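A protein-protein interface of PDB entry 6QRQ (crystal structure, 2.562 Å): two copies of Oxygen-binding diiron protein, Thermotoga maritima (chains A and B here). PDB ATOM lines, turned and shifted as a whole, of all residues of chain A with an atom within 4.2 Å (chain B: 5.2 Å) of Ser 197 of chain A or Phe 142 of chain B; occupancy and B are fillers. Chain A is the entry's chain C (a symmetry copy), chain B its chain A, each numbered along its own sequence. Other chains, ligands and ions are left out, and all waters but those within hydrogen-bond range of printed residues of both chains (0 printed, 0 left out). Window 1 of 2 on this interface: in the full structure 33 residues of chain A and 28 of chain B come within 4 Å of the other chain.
ND1 of His 141 of chain B sits at hydrogen-bond distance from NH2 of Arg 194 of chain A, at 3.3 Å.
The guanidinium group of Arg 194 of chain A is in hydrogen-bond range of the backbone carbonyl oxygen of Thr 146 of chain B.
The backbone carbonyl oxygen of Phe 142 of chain A is in hydrogen-bond range of the side-chain hydroxyl of Ser 197 of chain A, at 3.2 Å.
The backbone NH of Val 244 of chain A sits at hydrogen-bond distance from the backbone carbonyl oxygen of Ser 197 of chain A (2.8 Å).
N of Ala 201 of chain B sits at hydrogen-bond distance from OG of Ser 198 of chain B (3.4 Å).
The backbone carbonyl oxygen (O) of Ser 198 of chain A lies close to the side-chain sulfur (SG) of Cys 242 of chain A, 3.7 Å away.
The backbone NH (N) of Gly 243 of chain A lies within hydrogen-bond range of the backbone carbonyl oxygen (O) of Met 196 of chain A, at 3.1 Å.
O of Ser 197 of chain B sits at hydrogen-bond distance from N of Val 244 of chain B, at 2.8 Å.
Phe 142 of chain A touches Tyr 195 of chain B.
OG of Ser 197 of chain B touches CD1 of Phe 142 of chain A, 3.9 Å away.
Phe 142 of chain A touches Val 244 of chain B.
Arg 194 of chain A touches Phe 142 of chain B (O to CZ, 3.4 Å).
Ser 197 of chain B touches Ser 197 of chain A (OG to OG, 3.5 Å).
Gly 243 of chain A touches Phe 142 of chain B (CA to CZ, 3.5 Å).
OG of Ser 198 of chain B touches CG1 of Val 244 of chain A, at 3.8 Å.
CG1 of Val 244 of chain A touches N of Ala 201 of chain B (3.7 Å).
Ile 247 of chain A touches His 141 of chain B (CD1 to O, 3.97 Å).
Leu 250 of chain A touches Phe 142 of chain B.
Printed residues of chain B within 4 Å of Arg 194 of chain A: His 141, Phe 142 and Thr 146.
Ser 197 of chain A touches just these residues of chain B: Phe 142 and Ser 197.
Cys 242 of chain A touches none of the printed residues of chain B.
Of chain A, only Arg 194, Tyr 195, Ser 197, Gly 243, Val 244 and Leu 250 come within 4 Å of Phe 142 of chain B.
Met 196 of chain B touches none of the printed residues of chain A.
Of the printed residues of chain A, Ser 197 of chain B touches Phe 142 and Ser 197.
Printed residues of chain A within 4 Å of Ala 201 of chain B: Val 244 (3.7 Å).
Hydrophobic or aromatic side chains of chain B within 4 Å of the printed part of chain A: His 141, Phe 142 and Val 244.
Of the 11 printed residues of chain A, 9 touch a printed residue of chain B.
Printed residues of chain A that touch a printed residue of chain B: Phe 142, Arg 194, Tyr 195, Ser 197, Ser 198, Gly 243, Val 244, Ile 247 and Leu 250.
Among the printed residues, 17 pairs touch across the chains.
Phe 142 of chain A touches Ser 197 of chain B, and with the chains exchanged Ser 197 of chain A touches Phe 142 of chain B.
Phe 142 of chain A touches Val 244 of chain B, and with the chains exchanged Val 244 of chain A touches Phe 142 of chain B.
Ser 197 of chain B touches its own counterpart, Ser 197 of chain A.
Ser 198 of chain A touches Val 244 of chain B, and with the chains exchanged Val 244 of chain A touches Ser 198 of chain B.
Positions printed for both chains: 142, 195, 196, 197, 198 and 244.
Of the 17 pairs that touch across the chains among the printed residues, 9 have their exchanged pair printed and touching as well.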
ATOM      1  N   PHE A 142       7.687   9.881  21.220  1.00  0.00           N
ATOM      2  CA  PHE A 142       7.103   8.592  21.605  1.00  0.00           C
ATOM      3  C   PHE A 142       8.176   7.614  22.070  1.00  0.00           C
ATOM      4  O   PHE A 142       7.884   6.424  22.250  1.00  0.00           O
ATOM      5  CB  PHE A 142       6.236   7.982  20.488  1.00  0.00           C
ATOM      6  CG  PHE A 142       5.071   8.874  20.088  1.00  0.00           C
ATOM      7  CD1 PHE A 142       3.989   9.050  20.943  1.00  0.00           C
ATOM      8  CD2 PHE A 142       5.089   9.583  18.891  1.00  0.00           C
ATOM      9  CE1 PHE A 142       2.937   9.895  20.599  1.00  0.00           C
ATOM     10  CE2 PHE A 142       4.044  10.432  18.536  1.00  0.00           C
ATOM     11  CZ  PHE A 142       2.975  10.596  19.383  1.00  0.00           C
ATOM     12  N   ARG A 194       8.432  -1.860  27.996  1.00  0.00           N
ATOM     13  CA  ARG A 194       7.250  -1.261  28.607  1.00  0.00           C
ATOM     14  C   ARG A 194       7.035   0.177  28.176  1.00  0.00           C
ATOM     15  O   ARG A 194       5.885   0.601  28.038  1.00  0.00           O
ATOM     16  CB  ARG A 194       7.340  -1.329  30.134  1.00  0.00           C
ATOM     17  CG  ARG A 194       6.149  -0.744  30.871  1.00  0.00           C
ATOM     18  CD  ARG A 194       4.813  -1.342  30.408  1.00  0.00           C
ATOM     19  NE  ARG A 194       3.665  -0.756  31.106  1.00  0.00           N
ATOM     20  CZ  ARG A 194       2.977   0.306  30.683  1.00  0.00           C
ATOM     21  NH1 ARG A 194       3.308   0.911  29.558  1.00  0.00           N
ATOM     22  NH2 ARG A 194       1.958   0.772  31.384  1.00  0.00           N
ATOM     23  N   TYR A 195       8.117   0.933  27.965  1.00  0.00           N
ATOM     24  CA  TYR A 195       8.066   2.386  27.803  1.00  0.00           C
ATOM     25  C   TYR A 195       8.110   2.875  26.352  1.00  0.00           C
ATOM     26  O   TYR A 195       7.444   3.861  26.032  1.00  0.00           O
ATOM     27  CB  TYR A 195       9.206   3.023  28.597  1.00  0.00           C
ATOM     28  CG  TYR A 195       8.884   3.339  30.047  1.00  0.00           C
ATOM     29  CD1 TYR A 195       8.819   2.322  30.998  1.00  0.00           C
ATOM     30  CD2 TYR A 195       8.672   4.647  30.471  1.00  0.00           C
ATOM     31  CE1 TYR A 195       8.544   2.588  32.328  1.00  0.00           C
ATOM     32  CE2 TYR A 195       8.394   4.933  31.796  1.00  0.00           C
ATOM     33  CZ  TYR A 195       8.332   3.893  32.723  1.00  0.00           C
ATOM     34  OH  TYR A 195       8.060   4.117  34.060  1.00  0.00           O
ATOM     35  N   MET A 196       8.926   2.275  25.484  1.00  0.00           N
ATOM     36  CA  MET A 196       9.008   2.715  24.090  1.00  0.00           C
ATOM     37  C   MET A 196       7.733   2.345  23.321  1.00  0.00           C
ATOM     38  O   MET A 196       7.230   1.229  23.428  1.00  0.00           O
ATOM     39  CB  MET A 196      10.260   2.117  23.424  1.00  0.00           C
ATOM     40  CG  MET A 196      11.584   2.473  24.127  1.00  0.00           C
ATOM     41  SD  MET A 196      11.916   4.262  24.287  1.00  0.00           S
ATOM     42  CE  MET A 196      13.113   4.372  25.610  1.00  0.00           C
ATOM     43  N   SER A 197       7.225   3.280  22.512  1.00  0.00           N
ATOM     44  CA  SER A 197       5.826   3.205  22.083  1.00  0.00           C
ATOM     45  C   SER A 197       5.568   2.057  21.120  1.00  0.00           C
ATOM     46  O   SER A 197       4.551   1.360  21.240  1.00  0.00           O
ATOM     47  CB  SER A 197       5.388   4.515  21.428  1.00  0.00           C
ATOM     48  OG  SER A 197       4.863   5.398  22.397  1.00  0.00           O
ATOM     49  N   SER A 198       6.456   1.850  20.154  1.00  0.00           N
ATOM     50  CA  SER A 198       6.260   0.779  19.185  1.00  0.00           C
ATOM     51  C   SER A 198       7.541   0.605  18.403  1.00  0.00           C
ATOM     52  O   SER A 198       8.380   1.507  18.337  1.00  0.00           O
ATOM     53  CB  SER A 198       5.102   1.056  18.218  1.00  0.00           C
ATOM     54  OG  SER A 198       5.455   2.050  17.253  1.00  0.00           O
ATOM     55  N   CYS A 242       7.986  -3.286  21.305  1.00  0.00           N
ATOM     56  CA  CYS A 242       7.763  -2.531  22.535  1.00  0.00           C
ATOM     57  C   CYS A 242       6.354  -1.941  22.524  1.00  0.00           C
ATOM     58  O   CYS A 242       5.686  -1.883  21.492  1.00  0.00           O
ATOM     59  CB  CYS A 242       8.831  -1.442  22.748  1.00  0.00           C
ATOM     60  SG  CYS A 242       9.234  -0.670  21.231  1.00  0.00           S
ATOM     61  N   GLY A 243       5.899  -1.569  23.707  1.00  0.00           N
ATOM     62  CA  GLY A 243       4.766  -0.665  23.859  1.00  0.00           C
ATOM     63  C   GLY A 243       3.470  -1.275  23.334  1.00  0.00           C
ATOM     64  O   GLY A 243       3.000  -2.317  23.810  1.00  0.00           O
ATOM     65  N   VAL A 244       2.862  -0.593  22.361  1.00  0.00           N
ATOM     66  CA  VAL A 244       1.618  -1.033  21.736  1.00  0.00           C
ATOM     67  C   VAL A 244       1.787  -2.363  21.008  1.00  0.00           C
ATOM     68  O   VAL A 244       0.815  -3.115  20.863  1.00  0.00           O
ATOM     69  CB  VAL A 244       1.116   0.067  20.773  1.00  0.00           C
ATOM     70  CG1 VAL A 244      -0.217  -0.303  20.142  1.00  0.00           C
ATOM     71  CG2 VAL A 244       1.011   1.393  21.513  1.00  0.00           C
ATOM     72  N   ILE A 247       0.596  -4.797  23.460  1.00  0.00           N
ATOM     73  CA  ILE A 247      -0.469  -4.223  24.270  1.00  0.00           C
ATOM     74  C   ILE A 247      -1.548  -5.237  24.614  1.00  0.00           C
ATOM     75  O   ILE A 247      -2.424  -4.933  25.434  1.00  0.00           O
ATOM     76  CB  ILE A 247      -1.057  -2.986  23.575  1.00  0.00           C
ATOM     77  CG1 ILE A 247      -1.636  -2.020  24.624  1.00  0.00           C
ATOM     78  CG2 ILE A 247      -2.054  -3.398  22.500  1.00  0.00           C
ATOM     79  CD1 ILE A 247      -1.906  -0.613  24.098  1.00  0.00           C
ATOM     80  N   LEU A 250      -0.258  -6.045  27.983  1.00  0.00           N
ATOM     81  CA  LEU A 250      -0.895  -4.986  28.745  1.00  0.00           C
ATOM     82  C   LEU A 250      -2.408  -5.178  28.592  1.00  0.00           C
ATOM     83  O   LEU A 250      -2.871  -5.946  27.742  1.00  0.00           O
ATOM     84  CB  LEU A 250      -0.440  -3.607  28.254  1.00  0.00           C
ATOM     85  CG  LEU A 250       1.054  -3.277  28.092  1.00  0.00           C
ATOM     86  CD1 LEU A 250       1.251  -1.804  27.789  1.00  0.00           C
ATOM     87  CD2 LEU A 250       1.812  -3.644  29.335  1.00  0.00           C
ATOM     88  N   ALA B 140      -5.580   2.069  29.571  1.00  0.00           N
ATOM     89  CA  ALA B 140      -5.653   2.982  28.440  1.00  0.00           C
ATOM     90  C   ALA B 140      -4.253   3.456  28.120  1.00  0.00           C
ATOM     91  O   ALA B 140      -4.029   4.627  27.805  1.00  0.00           O
ATOM     92  CB  ALA B 140      -6.577   4.170  28.712  1.00  0.00           C
ATOM     93  N   HIS B 141      -3.285   2.554  28.242  1.00  0.00           N
ATOM     94  CA  HIS B 141      -1.889   2.943  28.127  1.00  0.00           C
ATOM     95  C   HIS B 141      -1.627   3.452  26.723  1.00  0.00           C
ATOM     96  O   HIS B 141      -2.226   2.985  25.750  1.00  0.00           O
ATOM     97  CB  HIS B 141      -0.982   1.752  28.461  1.00  0.00           C
ATOM     98  CG  HIS B 141      -1.309   1.111  29.778  1.00  0.00           C
ATOM     99  ND1 HIS B 141      -1.168   1.771  30.985  1.00  0.00           N
ATOM    100  CD2 HIS B 141      -1.807  -0.117  30.073  1.00  0.00           C
ATOM    101  CE1 HIS B 141      -1.567   0.976  31.964  1.00  0.00           C
ATOM    102  NE2 HIS B 141      -1.960  -0.175  31.435  1.00  0.00           N
ATOM    103  N   PHE B 142      -0.796   4.478  26.633  1.00  0.00           N
ATOM    104  CA  PHE B 142      -0.355   5.080  25.387  1.00  0.00           C
ATOM    105  C   PHE B 142      -1.448   5.950  24.786  1.00  0.00           C
ATOM    106  O   PHE B 142      -1.287   6.445  23.674  1.00  0.00           O
ATOM    107  CB  PHE B 142       0.126   4.018  24.393  1.00  0.00           C
ATOM    108  CG  PHE B 142       1.274   3.206  24.926  1.00  0.00           C
ATOM    109  CD1 PHE B 142       2.521   3.787  25.086  1.00  0.00           C
ATOM    110  CD2 PHE B 142       1.089   1.897  25.337  1.00  0.00           C
ATOM    111  CE1 PHE B 142       3.573   3.072  25.609  1.00  0.00           C
ATOM    112  CE2 PHE B 142       2.141   1.161  25.875  1.00  0.00           C
ATOM    113  CZ  PHE B 142       3.386   1.750  26.013  1.00  0.00           C
ATOM    114  N   LEU B 143      -2.525   6.213  25.523  1.00  0.00           N
ATOM    115  CA  LEU B 143      -3.579   7.106  25.060  1.00  0.00           C
ATOM    116  C   LEU B 143      -3.864   8.157  26.139  1.00  0.00           C
ATOM    117  O   LEU B 143      -4.976   8.238  26.660  1.00  0.00           O
ATOM    118  CB  LEU B 143      -4.851   6.331  24.718  1.00  0.00           C
ATOM    119  CG  LEU B 143      -4.791   5.085  23.835  1.00  0.00           C
ATOM    120  CD1 LEU B 143      -6.107   4.311  23.973  1.00  0.00           C
ATOM    121  CD2 LEU B 143      -4.562   5.459  22.386  1.00  0.00           C
ATOM    122  N   HIS B 144      -2.881   9.008  26.445  1.00  0.00           N
ATOM    123  CA  HIS B 144      -1.635   9.149  25.688  1.00  0.00           C
ATOM    124  C   HIS B 144      -0.424   8.667  26.503  1.00  0.00           C
ATOM    125  O   HIS B 144       0.616   8.295  25.933  1.00  0.00           O
ATOM    126  CB  HIS B 144      -1.444  10.605  25.233  1.00  0.00           C
ATOM    127  CG  HIS B 144      -1.733  11.617  26.300  1.00  0.00           C
ATOM    128  ND1 HIS B 144      -0.767  12.082  27.170  1.00  0.00           N
ATOM    129  CD2 HIS B 144      -2.880  12.255  26.635  1.00  0.00           C
ATOM    130  CE1 HIS B 144      -1.310  12.958  27.999  1.00  0.00           C
ATOM    131  NE2 HIS B 144      -2.589  13.087  27.691  1.00  0.00           N
ATOM    132  N   SER B 145      -0.563   8.699  27.827  1.00  0.00           N
ATOM    133  CA  SER B 145       0.554   8.419  28.714  1.00  0.00           C
ATOM    134  C   SER B 145       0.930   6.950  28.675  1.00  0.00           C
ATOM    135  O   SER B 145       0.083   6.076  28.497  1.00  0.00           O
ATOM    136  CB  SER B 145       0.199   8.768  30.160  1.00  0.00           C
ATOM    137  OG  SER B 145       0.134  10.162  30.331  1.00  0.00           O
ATOM    138  N   THR B 146       2.220   6.699  28.909  1.00  0.00           N
ATOM    139  CA  THR B 146       2.775   5.352  28.957  1.00  0.00           C
ATOM    140  C   THR B 146       2.067   4.500  30.003  1.00  0.00           C
ATOM    141  O   THR B 146       1.808   3.314  29.772  1.00  0.00           O
ATOM    142  CB  THR B 146       4.270   5.446  29.244  1.00  0.00           C
ATOM    143  OG1 THR B 146       4.884   6.252  28.229  1.00  0.00           O
ATOM    144  CG2 THR B 146       4.928   4.058  29.286  1.00  0.00           C
ATOM    145  N   ASN B 148      -1.527   4.725  31.739  1.00  0.00           N
ATOM    146  CA  ASN B 148      -2.727   5.547  31.625  1.00  0.00           C
ATOM    147  C   ASN B 148      -3.966   4.688  31.833  1.00  0.00           C
ATOM    148  O   ASN B 148      -4.002   3.506  31.454  1.00  0.00           O
ATOM    149  CB  ASN B 148      -2.755   6.275  30.263  1.00  0.00           C
ATOM    150  CG  ASN B 148      -3.853   7.322  30.169  1.00  0.00           C
ATOM    151  OD1 ASN B 148      -3.931   8.253  30.975  1.00  0.00           O
ATOM    152  ND2 ASN B 148      -4.708   7.173  29.173  1.00  0.00           N
ATOM    153  N   TYR B 195      -1.323  13.381  20.097  1.00  0.00           N
ATOM    154  CA  TYR B 195      -1.064  12.739  21.385  1.00  0.00           C
ATOM    155  C   TYR B 195      -1.288  11.235  21.424  1.00  0.00           C
ATOM    156  O   TYR B 195      -0.533  10.538  22.099  1.00  0.00           O
ATOM    157  CB  TYR B 195      -1.930  13.373  22.467  1.00  0.00           C
ATOM    158  CG  TYR B 195      -1.279  14.563  23.105  1.00  0.00           C
ATOM    159  CD1 TYR B 195      -1.237  15.787  22.444  1.00  0.00           C
ATOM    160  CD2 TYR B 195      -0.704  14.470  24.371  1.00  0.00           C
ATOM    161  CE1 TYR B 195      -0.668  16.879  23.021  1.00  0.00           C
ATOM    162  CE2 TYR B 195      -0.126  15.553  24.953  1.00  0.00           C
ATOM    163  CZ  TYR B 195      -0.106  16.761  24.275  1.00  0.00           C
ATOM    164  OH  TYR B 195       0.477  17.867  24.857  1.00  0.00           O
ATOM    165  N   MET B 196      -2.345  10.717  20.806  1.00  0.00           N
ATOM    166  CA  MET B 196      -2.632   9.289  20.908  1.00  0.00           C
ATOM    167  C   MET B 196      -1.585   8.489  20.141  1.00  0.00           C
ATOM    168  O   MET B 196      -1.206   8.855  19.029  1.00  0.00           O
ATOM    169  CB  MET B 196      -4.049   9.014  20.405  1.00  0.00           C
ATOM    170  CG  MET B 196      -5.105   9.869  21.111  1.00  0.00           C
ATOM    171  SD  MET B 196      -5.145   9.564  22.909  1.00  0.00           S
ATOM    172  CE  MET B 196      -5.812  11.090  23.569  1.00  0.00           C
ATOM    173  N   SER B 197      -1.113   7.390  20.741  1.00  0.00           N
ATOM    174  CA  SER B 197       0.168   6.808  20.326  1.00  0.00           C
ATOM    175  C   SER B 197       0.101   6.169  18.939  1.00  0.00           C
ATOM    176  O   SER B 197       1.065   6.266  18.169  1.00  0.00           O
ATOM    177  CB  SER B 197       0.648   5.777  21.348  1.00  0.00           C
ATOM    178  OG  SER B 197       1.504   6.384  22.306  1.00  0.00           O
ATOM    179  N   SER B 198      -0.986   5.468  18.624  1.00  0.00           N
ATOM    180  CA  SER B 198      -1.152   4.821  17.323  1.00  0.00           C
ATOM    181  C   SER B 198      -2.588   4.329  17.205  1.00  0.00           C
ATOM    182  O   SER B 198      -3.269   4.114  18.213  1.00  0.00           O
ATOM    183  CB  SER B 198      -0.182   3.657  17.126  1.00  0.00           C
ATOM    184  OG  SER B 198      -0.778   2.458  17.574  1.00  0.00           O
ATOM    185  N   ALA B 201      -3.474   1.308  19.243  1.00  0.00           N
ATOM    186  CA  ALA B 201      -3.840   1.534  20.645  1.00  0.00           C
ATOM    187  C   ALA B 201      -5.282   2.026  20.785  1.00  0.00           C
ATOM    188  O   ALA B 201      -5.989   1.629  21.723  1.00  0.00           O
ATOM    189  CB  ALA B 201      -2.862   2.527  21.283  1.00  0.00           C
ATOM    190  N   VAL B 244       2.350   7.844  16.269  1.00  0.00           N
ATOM    191  CA  VAL B 244       3.404   7.221  15.462  1.00  0.00           C
ATOM    192  C   VAL B 244       2.952   6.989  14.027  1.00  0.00           C
ATOM    193  O   VAL B 244       3.785   6.946  13.111  1.00  0.00           O
ATOM    194  CB  VAL B 244       3.880   5.903  16.104  1.00  0.00           C
ATOM    195  CG1 VAL B 244       5.052   5.327  15.329  1.00  0.00           C
ATOM    196  CG2 VAL B 244       4.270   6.096  17.589  1.00  0.00           C
